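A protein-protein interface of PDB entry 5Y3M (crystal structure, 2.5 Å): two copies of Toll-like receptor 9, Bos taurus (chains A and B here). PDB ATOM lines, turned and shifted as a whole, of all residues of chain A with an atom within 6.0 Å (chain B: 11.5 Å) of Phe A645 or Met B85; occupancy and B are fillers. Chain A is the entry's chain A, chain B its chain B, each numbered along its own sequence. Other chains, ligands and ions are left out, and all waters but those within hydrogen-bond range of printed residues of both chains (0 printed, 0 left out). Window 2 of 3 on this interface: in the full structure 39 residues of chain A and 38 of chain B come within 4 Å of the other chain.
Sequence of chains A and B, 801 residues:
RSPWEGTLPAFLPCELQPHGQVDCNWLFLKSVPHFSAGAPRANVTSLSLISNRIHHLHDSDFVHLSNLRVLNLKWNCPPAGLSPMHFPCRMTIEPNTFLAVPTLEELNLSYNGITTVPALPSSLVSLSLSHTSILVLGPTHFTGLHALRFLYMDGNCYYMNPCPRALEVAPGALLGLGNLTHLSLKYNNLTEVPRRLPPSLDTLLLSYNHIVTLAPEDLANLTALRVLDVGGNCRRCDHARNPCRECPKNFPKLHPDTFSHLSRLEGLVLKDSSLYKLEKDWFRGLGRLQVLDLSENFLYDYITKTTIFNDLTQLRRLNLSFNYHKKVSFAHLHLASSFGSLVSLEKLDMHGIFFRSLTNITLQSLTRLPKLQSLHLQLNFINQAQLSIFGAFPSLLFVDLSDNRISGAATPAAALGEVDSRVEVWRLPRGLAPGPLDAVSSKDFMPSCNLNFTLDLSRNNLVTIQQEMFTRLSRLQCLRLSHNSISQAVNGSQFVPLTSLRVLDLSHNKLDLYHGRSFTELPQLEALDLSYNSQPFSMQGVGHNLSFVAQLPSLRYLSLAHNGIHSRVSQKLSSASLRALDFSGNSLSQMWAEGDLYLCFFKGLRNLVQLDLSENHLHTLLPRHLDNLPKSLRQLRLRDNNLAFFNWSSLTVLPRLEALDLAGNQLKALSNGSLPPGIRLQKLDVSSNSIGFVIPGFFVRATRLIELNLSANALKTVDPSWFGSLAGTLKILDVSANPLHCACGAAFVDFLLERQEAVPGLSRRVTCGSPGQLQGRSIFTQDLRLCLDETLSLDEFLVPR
Hydrophobic or aromatic side chains of chain A within 4 Å of the printed part of chain B: Leu A622 and Phe A645.
Printed residues of chain B that touch a printed residue of chain A: Pro B84, Met B85 and His B86.
Hydrophobic or aromatic side chains of chain B within 4 Å of the printed part of chain A: Met B85 and His B86.
Among the printed residues, 7 pairs touch across the chains.
Among the printed residues, no Asp or Glu carboxylate lies within 4 Å of a Lys or Arg side-chain nitrogen of the other chain.
Phe A645 touches just one residue of chain B: Met B85.
Of chain A, only Thr A620, Leu A622 and Phe A645 come within 4 Å of Met B85.
Thr A620 touches just these residues of chain B: Pro B84 (3.8 Å) and Met B85 (3.6 Å).
No residue of chain B comes within 4 Å of Leu A643.
No residue of chain B comes within 4 Å of Ala A644.
No residue of chain B comes within 4 Å of Phe A646.
No residue of chain B comes within 4 Å of Asn A672.
Printed residues of chain A within 4 Å of Pro B84: Thr A620 (3.8 Å) and Leu A622 (3.8 Å).
Printed residues of chain B within 4 Å of Arg A624: His B86.
Of the printed residues of chain B, Leu A622 touches Pro B84 (3.8 Å), Met B85 (3.8 Å) and His B86 (3.5 Å).
Printed residues of chain A within 4 Å of His B86: Leu A622 and Arg A624.
Arg B53 touches none of the printed residues of chain A.
Gly B81 touches none of the printed residues of chain A.
The nearest residue of chain B that does not touch Phe A645 is Phe B87 (6.1 Å).
The nearest printed residue of chain A that does not touch Met B85 is Arg A624 (5.3 Å).
The nearest printed residue of chain A that does not touch His B86 is Thr A620 (6.9 Å).
No position is printed for both chains.
Thr A620 touches Pro B84.
CD2 of Leu A622 touches O of Pro B84, 3.8 Å away.
Leu A622 touches Met B85.
His B86 touches Leu A622.
Arg A624 touches His B86.
Phe A645 touches Met B85 (CE1 to CE, 3.5 Å).
OG1 of Thr A620 is in hydrogen-bond range of SD of Met B85 (3.6 Å).
The backbone carbonyl oxygen of Ala B80 sits at hydrogen-bond distance from a ring nitrogen (ND1) of His B86 (3.0 Å).
SG of Cys B89 forms a disulfide with SG of Cys B77 (2.0 Å).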
ATOM      1  N   HIS A 619      28.346 -32.689  21.776  1.00  0.00           N
ATOM      2  CA  HIS A 619      27.498 -33.335  22.787  1.00  0.00           C
ATOM      3  C   HIS A 619      26.084 -32.747  22.823  1.00  0.00           C
ATOM      4  O   HIS A 619      25.138 -33.438  23.205  1.00  0.00           O
ATOM      5  CB  HIS A 619      28.135 -33.234  24.177  1.00  0.00           C
ATOM      6  CG  HIS A 619      29.388 -34.044  24.328  1.00  0.00           C
ATOM      7  ND1 HIS A 619      29.385 -35.347  24.783  1.00  0.00           N
ATOM      8  CD2 HIS A 619      30.687 -33.731  24.089  1.00  0.00           C
ATOM      9  CE1 HIS A 619      30.626 -35.801  24.819  1.00  0.00           C
ATOM     10  NE2 HIS A 619      31.435 -34.842  24.400  1.00  0.00           N
ATOM     11  N   THR A 620      25.956 -31.482  22.422  1.00  0.00           N
ATOM     12  CA  THR A 620      24.691 -30.742  22.460  1.00  0.00           C
ATOM     13  C   THR A 620      24.545 -29.907  21.187  1.00  0.00           C
ATOM     14  O   THR A 620      25.535 -29.506  20.582  1.00  0.00           O
ATOM     15  CB  THR A 620      24.600 -29.844  23.716  1.00  0.00           C
ATOM     16  OG1 THR A 620      23.484 -28.958  23.605  1.00  0.00           O
ATOM     17  CG2 THR A 620      25.856 -29.021  23.897  1.00  0.00           C
ATOM     18  N   LEU A 621      23.302 -29.671  20.777  1.00  0.00           N
ATOM     19  CA  LEU A 621      23.006 -28.930  19.551  1.00  0.00           C
ATOM     20  C   LEU A 621      21.716 -28.129  19.713  1.00  0.00           C
ATOM     21  O   LEU A 621      20.620 -28.662  19.581  1.00  0.00           O
ATOM     22  CB  LEU A 621      22.911 -29.895  18.369  1.00  0.00           C
ATOM     23  CG  LEU A 621      22.923 -29.298  16.963  1.00  0.00           C
ATOM     24  CD1 LEU A 621      24.207 -28.541  16.659  1.00  0.00           C
ATOM     25  CD2 LEU A 621      22.728 -30.407  15.946  1.00  0.00           C
ATOM     26  N   LEU A 622      21.873 -26.837  19.997  1.00  0.00           N
ATOM     27  CA  LEU A 622      20.773 -25.975  20.437  1.00  0.00           C
ATOM     28  C   LEU A 622      20.054 -25.279  19.285  1.00  0.00           C
ATOM     29  O   LEU A 622      20.606 -25.177  18.188  1.00  0.00           O
ATOM     30  CB  LEU A 622      21.308 -24.900  21.379  1.00  0.00           C
ATOM     31  CG  LEU A 622      22.114 -25.384  22.588  1.00  0.00           C
ATOM     32  CD1 LEU A 622      22.747 -24.199  23.295  1.00  0.00           C
ATOM     33  CD2 LEU A 622      21.249 -26.194  23.544  1.00  0.00           C
ATOM     34  N   ARG A 624      19.583 -22.045  19.067  1.00  0.00           N
ATOM     35  CA  ARG A 624      20.618 -21.038  18.789  1.00  0.00           C
ATOM     36  C   ARG A 624      21.415 -21.339  17.528  1.00  0.00           C
ATOM     37  O   ARG A 624      21.467 -20.546  16.591  1.00  0.00           O
ATOM     38  CB  ARG A 624      21.637 -21.007  19.940  1.00  0.00           C
ATOM     39  CG  ARG A 624      21.401 -20.012  21.046  1.00  0.00           C
ATOM     40  CD  ARG A 624      22.582 -20.083  22.007  1.00  0.00           C
ATOM     41  NE  ARG A 624      22.384 -19.276  23.208  1.00  0.00           N
ATOM     42  CZ  ARG A 624      21.557 -19.581  24.211  1.00  0.00           C
ATOM     43  NH1 ARG A 624      21.465 -18.762  25.258  1.00  0.00           N
ATOM     44  NH2 ARG A 624      20.807 -20.689  24.183  1.00  0.00           N
ATOM     45  N   ASN A 642      28.756 -36.738  19.452  1.00  0.00           N
ATOM     46  CA  ASN A 642      28.452 -37.291  20.779  1.00  0.00           C
ATOM     47  C   ASN A 642      27.036 -36.924  21.264  1.00  0.00           C
ATOM     48  O   ASN A 642      26.823 -36.660  22.449  1.00  0.00           O
ATOM     49  CB  ASN A 642      29.522 -36.838  21.783  1.00  0.00           C
ATOM     50  CG  ASN A 642      30.916 -37.310  21.402  1.00  0.00           C
ATOM     51  OD1 ASN A 642      31.818 -36.509  21.166  1.00  0.00           O
ATOM     52  ND2 ASN A 642      31.092 -38.620  21.328  1.00  0.00           N
ATOM     53  N   LEU A 643      26.066 -36.951  20.349  1.00  0.00           N
ATOM     54  CA  LEU A 643      24.704 -36.487  20.640  1.00  0.00           C
ATOM     55  C   LEU A 643      23.840 -37.567  21.283  1.00  0.00           C
ATOM     56  O   LEU A 643      23.410 -38.499  20.611  1.00  0.00           O
ATOM     57  CB  LEU A 643      24.023 -35.965  19.366  1.00  0.00           C
ATOM     58  CG  LEU A 643      24.655 -34.739  18.710  1.00  0.00           C
ATOM     59  CD1 LEU A 643      24.109 -34.556  17.299  1.00  0.00           C
ATOM     60  CD2 LEU A 643      24.405 -33.497  19.548  1.00  0.00           C
ATOM     61  N   ALA A 644      23.594 -37.423  22.585  1.00  0.00           N
ATOM     62  CA  ALA A 644      22.697 -38.312  23.331  1.00  0.00           C
ATOM     63  C   ALA A 644      21.260 -37.782  23.415  1.00  0.00           C
ATOM     64  O   ALA A 644      20.373 -38.485  23.886  1.00  0.00           O
ATOM     65  CB  ALA A 644      23.254 -38.551  24.729  1.00  0.00           C
ATOM     66  N   PHE A 645      21.047 -36.547  22.969  1.00  0.00           N
ATOM     67  CA  PHE A 645      19.738 -35.891  22.985  1.00  0.00           C
ATOM     68  C   PHE A 645      19.623 -35.006  21.741  1.00  0.00           C
ATOM     69  O   PHE A 645      20.623 -34.455  21.272  1.00  0.00           O
ATOM     70  CB  PHE A 645      19.596 -35.045  24.263  1.00  0.00           C
ATOM     71  CG  PHE A 645      18.282 -34.314  24.385  1.00  0.00           C
ATOM     72  CD1 PHE A 645      18.143 -33.010  23.906  1.00  0.00           C
ATOM     73  CD2 PHE A 645      17.185 -34.920  24.992  1.00  0.00           C
ATOM     74  CE1 PHE A 645      16.934 -32.330  24.022  1.00  0.00           C
ATOM     75  CE2 PHE A 645      15.971 -34.245  25.102  1.00  0.00           C
ATOM     76  CZ  PHE A 645      15.848 -32.948  24.621  1.00  0.00           C
ATOM     77  N   PHE A 646      18.407 -34.881  21.212  1.00  0.00           N
ATOM     78  CA  PHE A 646      18.135 -33.984  20.086  1.00  0.00           C
ATOM     79  C   PHE A 646      16.715 -33.435  20.182  1.00  0.00           C
ATOM     80  O   PHE A 646      15.742 -34.202  20.212  1.00  0.00           O
ATOM     81  CB  PHE A 646      18.326 -34.722  18.762  1.00  0.00           C
ATOM     82  CG  PHE A 646      18.316 -33.825  17.558  1.00  0.00           C
ATOM     83  CD1 PHE A 646      17.116 -33.440  16.965  1.00  0.00           C
ATOM     84  CD2 PHE A 646      19.508 -33.378  17.000  1.00  0.00           C
ATOM     85  CE1 PHE A 646      17.104 -32.607  15.854  1.00  0.00           C
ATOM     86  CE2 PHE A 646      19.502 -32.550  15.881  1.00  0.00           C
ATOM     87  CZ  PHE A 646      18.299 -32.165  15.306  1.00  0.00           C
ATOM     88  N   ASN A 647      16.605 -32.108  20.210  1.00  0.00           N
ATOM     89  CA  ASN A 647      15.312 -31.420  20.272  1.00  0.00           C
ATOM     90  C   ASN A 647      14.707 -31.409  18.869  1.00  0.00           C
ATOM     91  O   ASN A 647      15.043 -30.561  18.047  1.00  0.00           O
ATOM     92  CB  ASN A 647      15.504 -29.991  20.820  1.00  0.00           C
ATOM     93  CG  ASN A 647      14.192 -29.242  21.021  1.00  0.00           C
ATOM     94  OD1 ASN A 647      13.105 -29.813  20.920  1.00  0.00           O
ATOM     95  ND2 ASN A 647      14.295 -27.945  21.323  1.00  0.00           N
ATOM     96  N   GLN A 666      24.607 -41.226  19.946  1.00  0.00           N
ATOM     97  CA  GLN A 666      24.184 -42.044  21.097  1.00  0.00           C
ATOM     98  C   GLN A 666      22.746 -41.762  21.545  1.00  0.00           C
ATOM     99  O   GLN A 666      22.450 -41.767  22.745  1.00  0.00           O
ATOM    100  CB  GLN A 666      25.148 -41.848  22.279  1.00  0.00           C
ATOM    101  CG  GLN A 666      26.580 -42.300  22.005  1.00  0.00           C
ATOM    102  CD  GLN A 666      27.416 -41.247  21.303  1.00  0.00           C
ATOM    103  OE1 GLN A 666      28.049 -41.510  20.276  1.00  0.00           O
ATOM    104  NE2 GLN A 666      27.412 -40.044  21.850  1.00  0.00           N
ATOM    105  N   LEU A 667      21.849 -41.546  20.581  1.00  0.00           N
ATOM    106  CA  LEU A 667      20.433 -41.339  20.884  1.00  0.00           C
ATOM    107  C   LEU A 667      19.840 -42.602  21.478  1.00  0.00           C
ATOM    108  O   LEU A 667      20.007 -43.675  20.912  1.00  0.00           O
ATOM    109  CB  LEU A 667      19.652 -40.949  19.627  1.00  0.00           C
ATOM    110  CG  LEU A 667      20.011 -39.631  18.946  1.00  0.00           C
ATOM    111  CD1 LEU A 667      19.292 -39.534  17.607  1.00  0.00           C
ATOM    112  CD2 LEU A 667      19.656 -38.459  19.846  1.00  0.00           C
ATOM    113  N   ASN A 672      10.732 -37.086  23.119  1.00  0.00           N
ATOM    114  CA  ASN A 672      10.920 -35.684  23.550  1.00  0.00           C
ATOM    115  C   ASN A 672      10.372 -34.756  22.461  1.00  0.00           C
ATOM    116  O   ASN A 672      11.099 -33.951  21.871  1.00  0.00           O
ATOM    117  CB  ASN A 672      12.395 -35.371  23.900  1.00  0.00           C
ATOM    118  CG  ASN A 672      12.983 -36.351  24.913  1.00  0.00           C
ATOM    119  OD1 ASN A 672      13.965 -37.039  24.622  1.00  0.00           O
ATOM    120  ND2 ASN A 672      12.385 -36.422  26.105  1.00  0.00           N
ATOM    121  N   PHE B  28      22.513 -39.543  38.644  1.00  0.00           N
ATOM    122  CA  PHE B  28      21.256 -38.853  38.278  1.00  0.00           C
ATOM    123  C   PHE B  28      20.239 -38.766  39.426  1.00  0.00           C
ATOM    124  O   PHE B  28      19.026 -38.815  39.218  1.00  0.00           O
ATOM    125  CB  PHE B  28      20.649 -39.486  37.012  1.00  0.00           C
ATOM    126  CG  PHE B  28      21.580 -39.463  35.833  1.00  0.00           C
ATOM    127  CD1 PHE B  28      21.612 -38.365  34.975  1.00  0.00           C
ATOM    128  CD2 PHE B  28      22.460 -40.521  35.601  1.00  0.00           C
ATOM    129  CE1 PHE B  28      22.485 -38.335  33.896  1.00  0.00           C
ATOM    130  CE2 PHE B  28      23.338 -40.494  34.531  1.00  0.00           C
ATOM    131  CZ  PHE B  28      23.347 -39.401  33.673  1.00  0.00           C
ATOM    132  N   ARG B  53      21.489 -34.497  39.992  1.00  0.00           N
ATOM    133  CA  ARG B  53      20.414 -33.518  39.764  1.00  0.00           C
ATOM    134  C   ARG B  53      19.763 -33.036  41.068  1.00  0.00           C
ATOM    135  O   ARG B  53      18.546 -32.853  41.135  1.00  0.00           O
ATOM    136  CB  ARG B  53      19.347 -34.136  38.863  1.00  0.00           C
ATOM    137  CG  ARG B  53      19.839 -34.356  37.460  1.00  0.00           C
ATOM    138  CD  ARG B  53      18.869 -35.142  36.614  1.00  0.00           C
ATOM    139  NE  ARG B  53      19.405 -35.275  35.258  1.00  0.00           N
ATOM    140  CZ  ARG B  53      18.752 -35.791  34.214  1.00  0.00           C
ATOM    141  NH1 ARG B  53      17.506 -36.248  34.342  1.00  0.00           N
ATOM    142  NH2 ARG B  53      19.363 -35.848  33.038  1.00  0.00           N
ATOM    143  N   TRP B  75      28.433 -29.255  40.357  1.00  0.00           N
ATOM    144  CA  TRP B  75      27.708 -29.484  39.079  1.00  0.00           C
ATOM    145  C   TRP B  75      26.267 -30.013  39.227  1.00  0.00           C
ATOM    146  O   TRP B  75      25.696 -30.531  38.272  1.00  0.00           O
ATOM    147  CB  TRP B  75      28.524 -30.404  38.120  1.00  0.00           C
ATOM    148  CG  TRP B  75      29.513 -29.674  37.236  1.00  0.00           C
ATOM    149  CD1 TRP B  75      30.882 -29.741  37.296  1.00  0.00           C
ATOM    150  CD2 TRP B  75      29.209 -28.780  36.160  1.00  0.00           C
ATOM    151  NE1 TRP B  75      31.442 -28.948  36.331  1.00  0.00           N
ATOM    152  CE2 TRP B  75      30.443 -28.345  35.615  1.00  0.00           C
ATOM    153  CE3 TRP B  75      28.014 -28.307  35.597  1.00  0.00           C
ATOM    154  CZ2 TRP B  75      30.516 -27.458  34.529  1.00  0.00           C
ATOM    155  CZ3 TRP B  75      28.087 -27.418  34.516  1.00  0.00           C
ATOM    156  CH2 TRP B  75      29.332 -27.005  33.999  1.00  0.00           C
ATOM    157  N   CYS B  77      23.381 -28.318  39.936  1.00  0.00           N
ATOM    158  CA  CYS B  77      22.315 -27.374  39.614  1.00  0.00           C
ATOM    159  C   CYS B  77      22.981 -26.197  38.910  1.00  0.00           C
ATOM    160  O   CYS B  77      22.985 -25.085  39.422  1.00  0.00           O
ATOM    161  CB  CYS B  77      21.588 -26.941  40.905  1.00  0.00           C
ATOM    162  SG  CYS B  77      20.260 -25.704  40.768  1.00  0.00           S
ATOM    163  N   PRO B  78      23.570 -26.454  37.726  1.00  0.00           N
ATOM    164  CA  PRO B  78      24.417 -25.435  37.100  1.00  0.00           C
ATOM    165  C   PRO B  78      23.613 -24.216  36.647  1.00  0.00           C
ATOM    166  O   PRO B  78      22.509 -24.384  36.122  1.00  0.00           O
ATOM    167  CB  PRO B  78      25.025 -26.164  35.903  1.00  0.00           C
ATOM    168  CG  PRO B  78      24.065 -27.264  35.587  1.00  0.00           C
ATOM    169  CD  PRO B  78      23.416 -27.652  36.877  1.00  0.00           C
ATOM    170  N   PRO B  79      24.145 -22.996  36.876  1.00  0.00           N
ATOM    171  CA  PRO B  79      23.475 -21.794  36.363  1.00  0.00           C
ATOM    172  C   PRO B  79      23.306 -21.819  34.838  1.00  0.00           C
ATOM    173  O   PRO B  79      24.032 -22.536  34.136  1.00  0.00           O
ATOM    174  CB  PRO B  79      24.409 -20.659  36.790  1.00  0.00           C
ATOM    175  CG  PRO B  79      25.146 -21.189  37.974  1.00  0.00           C
ATOM    176  CD  PRO B  79      25.292 -22.663  37.745  1.00  0.00           C
ATOM    177  N   ALA B  80      22.349 -21.031  34.352  1.00  0.00           N
ATOM    178  CA  ALA B  80      21.930 -21.044  32.945  1.00  0.00           C
ATOM    179  C   ALA B  80      23.099 -21.037  31.962  1.00  0.00           C
ATOM    180  O   ALA B  80      23.181 -21.890  31.085  1.00  0.00           O
ATOM    181  CB  ALA B  80      20.998 -19.872  32.661  1.00  0.00           C
ATOM    182  N   GLY B  81      24.015 -20.090  32.134  1.00  0.00           N
ATOM    183  CA  GLY B  81      25.154 -19.948  31.227  1.00  0.00           C
ATOM    184  C   GLY B  81      26.095 -21.147  31.167  1.00  0.00           C
ATOM    185  O   GLY B  81      26.727 -21.389  30.138  1.00  0.00           O
ATOM    186  N   LEU B  82      26.184 -21.886  32.274  1.00  0.00           N
ATOM    187  CA  LEU B  82      27.044 -23.066  32.394  1.00  0.00           C
ATOM    188  C   LEU B  82      26.329 -24.392  32.104  1.00  0.00           C
ATOM    189  O   LEU B  82      26.981 -25.422  31.896  1.00  0.00           O
ATOM    190  CB  LEU B  82      27.648 -23.101  33.799  1.00  0.00           C
ATOM    191  CG  LEU B  82      28.532 -21.888  34.099  1.00  0.00           C
ATOM    192  CD1 LEU B  82      28.588 -21.616  35.593  1.00  0.00           C
ATOM    193  CD2 LEU B  82      29.921 -22.072  33.487  1.00  0.00           C
ATOM    194  N   SER B  83      24.995 -24.373  32.130  1.00  0.00           N
ATOM    195  CA  SER B  83      24.180 -25.517  31.704  1.00  0.00           C
ATOM    196  C   SER B  83      24.381 -25.753  30.206  1.00  0.00           C
ATOM    197  O   SER B  83      24.254 -24.807  29.425  1.00  0.00           O
ATOM    198  CB  SER B  83      22.696 -25.253  31.988  1.00  0.00           C
ATOM    199  OG  SER B  83      21.863 -26.294  31.500  1.00  0.00           O
ATOM    200  N   PRO B  84      24.699 -26.998  29.794  1.00  0.00           N
ATOM    201  CA  PRO B  84      24.807 -27.337  28.361  1.00  0.00           C
ATOM    202  C   PRO B  84      23.626 -26.877  27.483  1.00  0.00           C
ATOM    203  O   PRO B  84      23.845 -26.385  26.372  1.00  0.00           O
ATOM    204  CB  PRO B  84      24.898 -28.865  28.375  1.00  0.00           C
ATOM    205  CG  PRO B  84      25.565 -29.179  29.671  1.00  0.00           C
ATOM    206  CD  PRO B  84      25.132 -28.123  30.647  1.00  0.00           C
ATOM    207  N   MET B  85      22.403 -27.026  27.996  1.00  0.00           N
ATOM    208  CA  MET B  85      21.171 -26.631  27.288  1.00  0.00           C
ATOM    209  C   MET B  85      20.657 -25.236  27.695  1.00  0.00           C
ATOM    210  O   MET B  85      19.569 -24.826  27.293  1.00  0.00           O
ATOM    211  CB  MET B  85      20.072 -27.671  27.538  1.00  0.00           C
ATOM    212  CG  MET B  85      20.452 -29.113  27.202  1.00  0.00           C
ATOM    213  SD  MET B  85      20.459 -29.520  25.450  1.00  0.00           S
ATOM    214  CE  MET B  85      18.714 -29.519  25.043  1.00  0.00           C
ATOM    215  N   HIS B  86      21.461 -24.512  28.475  1.00  0.00           N
ATOM    216  CA  HIS B  86      21.088 -23.230  29.088  1.00  0.00           C
ATOM    217  C   HIS B  86      19.797 -23.261  29.919  1.00  0.00           C
ATOM    218  O   HIS B  86      19.030 -22.298  29.938  1.00  0.00           O
ATOM    219  CB  HIS B  86      21.101 -22.106  28.043  1.00  0.00           C
ATOM    220  CG  HIS B  86      22.447 -21.891  27.423  1.00  0.00           C
ATOM    221  ND1 HIS B  86      23.516 -21.383  28.125  1.00  0.00           N
ATOM    222  CD2 HIS B  86      22.901 -22.135  26.172  1.00  0.00           C
ATOM    223  CE1 HIS B  86      24.571 -21.318  27.333  1.00  0.00           C
ATOM    224  NE2 HIS B  86      24.225 -21.769  26.141  1.00  0.00           N
ATOM    225  N   PHE B  87      19.589 -24.372  30.626  1.00  0.00           N
ATOM    226  CA  PHE B  87      18.480 -24.505  31.570  1.00  0.00           C
ATOM    227  C   PHE B  87      18.809 -23.706  32.833  1.00  0.00           C
ATOM    228  O   PHE B  87      19.882 -23.907  33.403  1.00  0.00           O
ATOM    229  CB  PHE B  87      18.268 -25.970  31.982  1.00  0.00           C
ATOM    230  CG  PHE B  87      17.823 -26.890  30.864  1.00  0.00           C
ATOM    231  CD1 PHE B  87      16.953 -26.463  29.847  1.00  0.00           C
ATOM    232  CD2 PHE B  87      18.232 -28.222  30.865  1.00  0.00           C
ATOM    233  CE1 PHE B  87      16.549 -27.334  28.844  1.00  0.00           C
ATOM    234  CE2 PHE B  87      17.820 -29.097  29.868  1.00  0.00           C
ATOM    235  CZ  PHE B  87      16.979 -28.655  28.857  1.00  0.00           C
ATOM    236  N   PRO B  88      17.899 -22.809  33.276  1.00  0.00           N
ATOM    237  CA  PRO B  88      18.143 -22.145  34.561  1.00  0.00           C
ATOM    238  C   PRO B  88      17.969 -23.113  35.727  1.00  0.00           C
ATOM    239  O   PRO B  88      17.206 -24.076  35.622  1.00  0.00           O
ATOM    240  CB  PRO B  88      17.088 -21.021  34.614  1.00  0.00           C
ATOM    241  CG  PRO B  88      16.199 -21.193  33.426  1.00  0.00           C
ATOM    242  CD  PRO B  88      16.594 -22.436  32.691  1.00  0.00           C
ATOM    243  N   CYS B  89      18.688 -22.860  36.815  1.00  0.00           N
ATOM    244  CA  CYS B  89      18.603 -23.692  38.007  1.00  0.00           C
ATOM    245  C   CYS B  89      18.819 -22.858  39.265  1.00  0.00           C
ATOM    246  O   CYS B  89      19.716 -22.010  39.316  1.00  0.00           O
ATOM    247  CB  CYS B  89      19.624 -24.830  37.944  1.00  0.00           C
ATOM    248  SG  CYS B  89      19.255 -26.195  39.070  1.00  0.00           S
ATOM    249  N   MET B 160      30.366 -16.600  30.538  1.00  0.00           N
ATOM    250  CA  MET B 160      29.802 -17.948  30.764  1.00  0.00           C
ATOM    251  C   MET B 160      28.831 -18.021  31.951  1.00  0.00           C
ATOM    252  O   MET B 160      28.091 -18.989  32.061  1.00  0.00           O
ATOM    253  CB  MET B 160      30.941 -18.969  30.981  1.00  0.00           C
ATOM    254  CG  MET B 160      30.836 -20.285  30.229  1.00  0.00           C
ATOM    255  SD  MET B 160      31.089 -20.127  28.445  1.00  0.00           S
ATOM    256  CE  MET B 160      29.397 -20.125  27.846  1.00  0.00           C
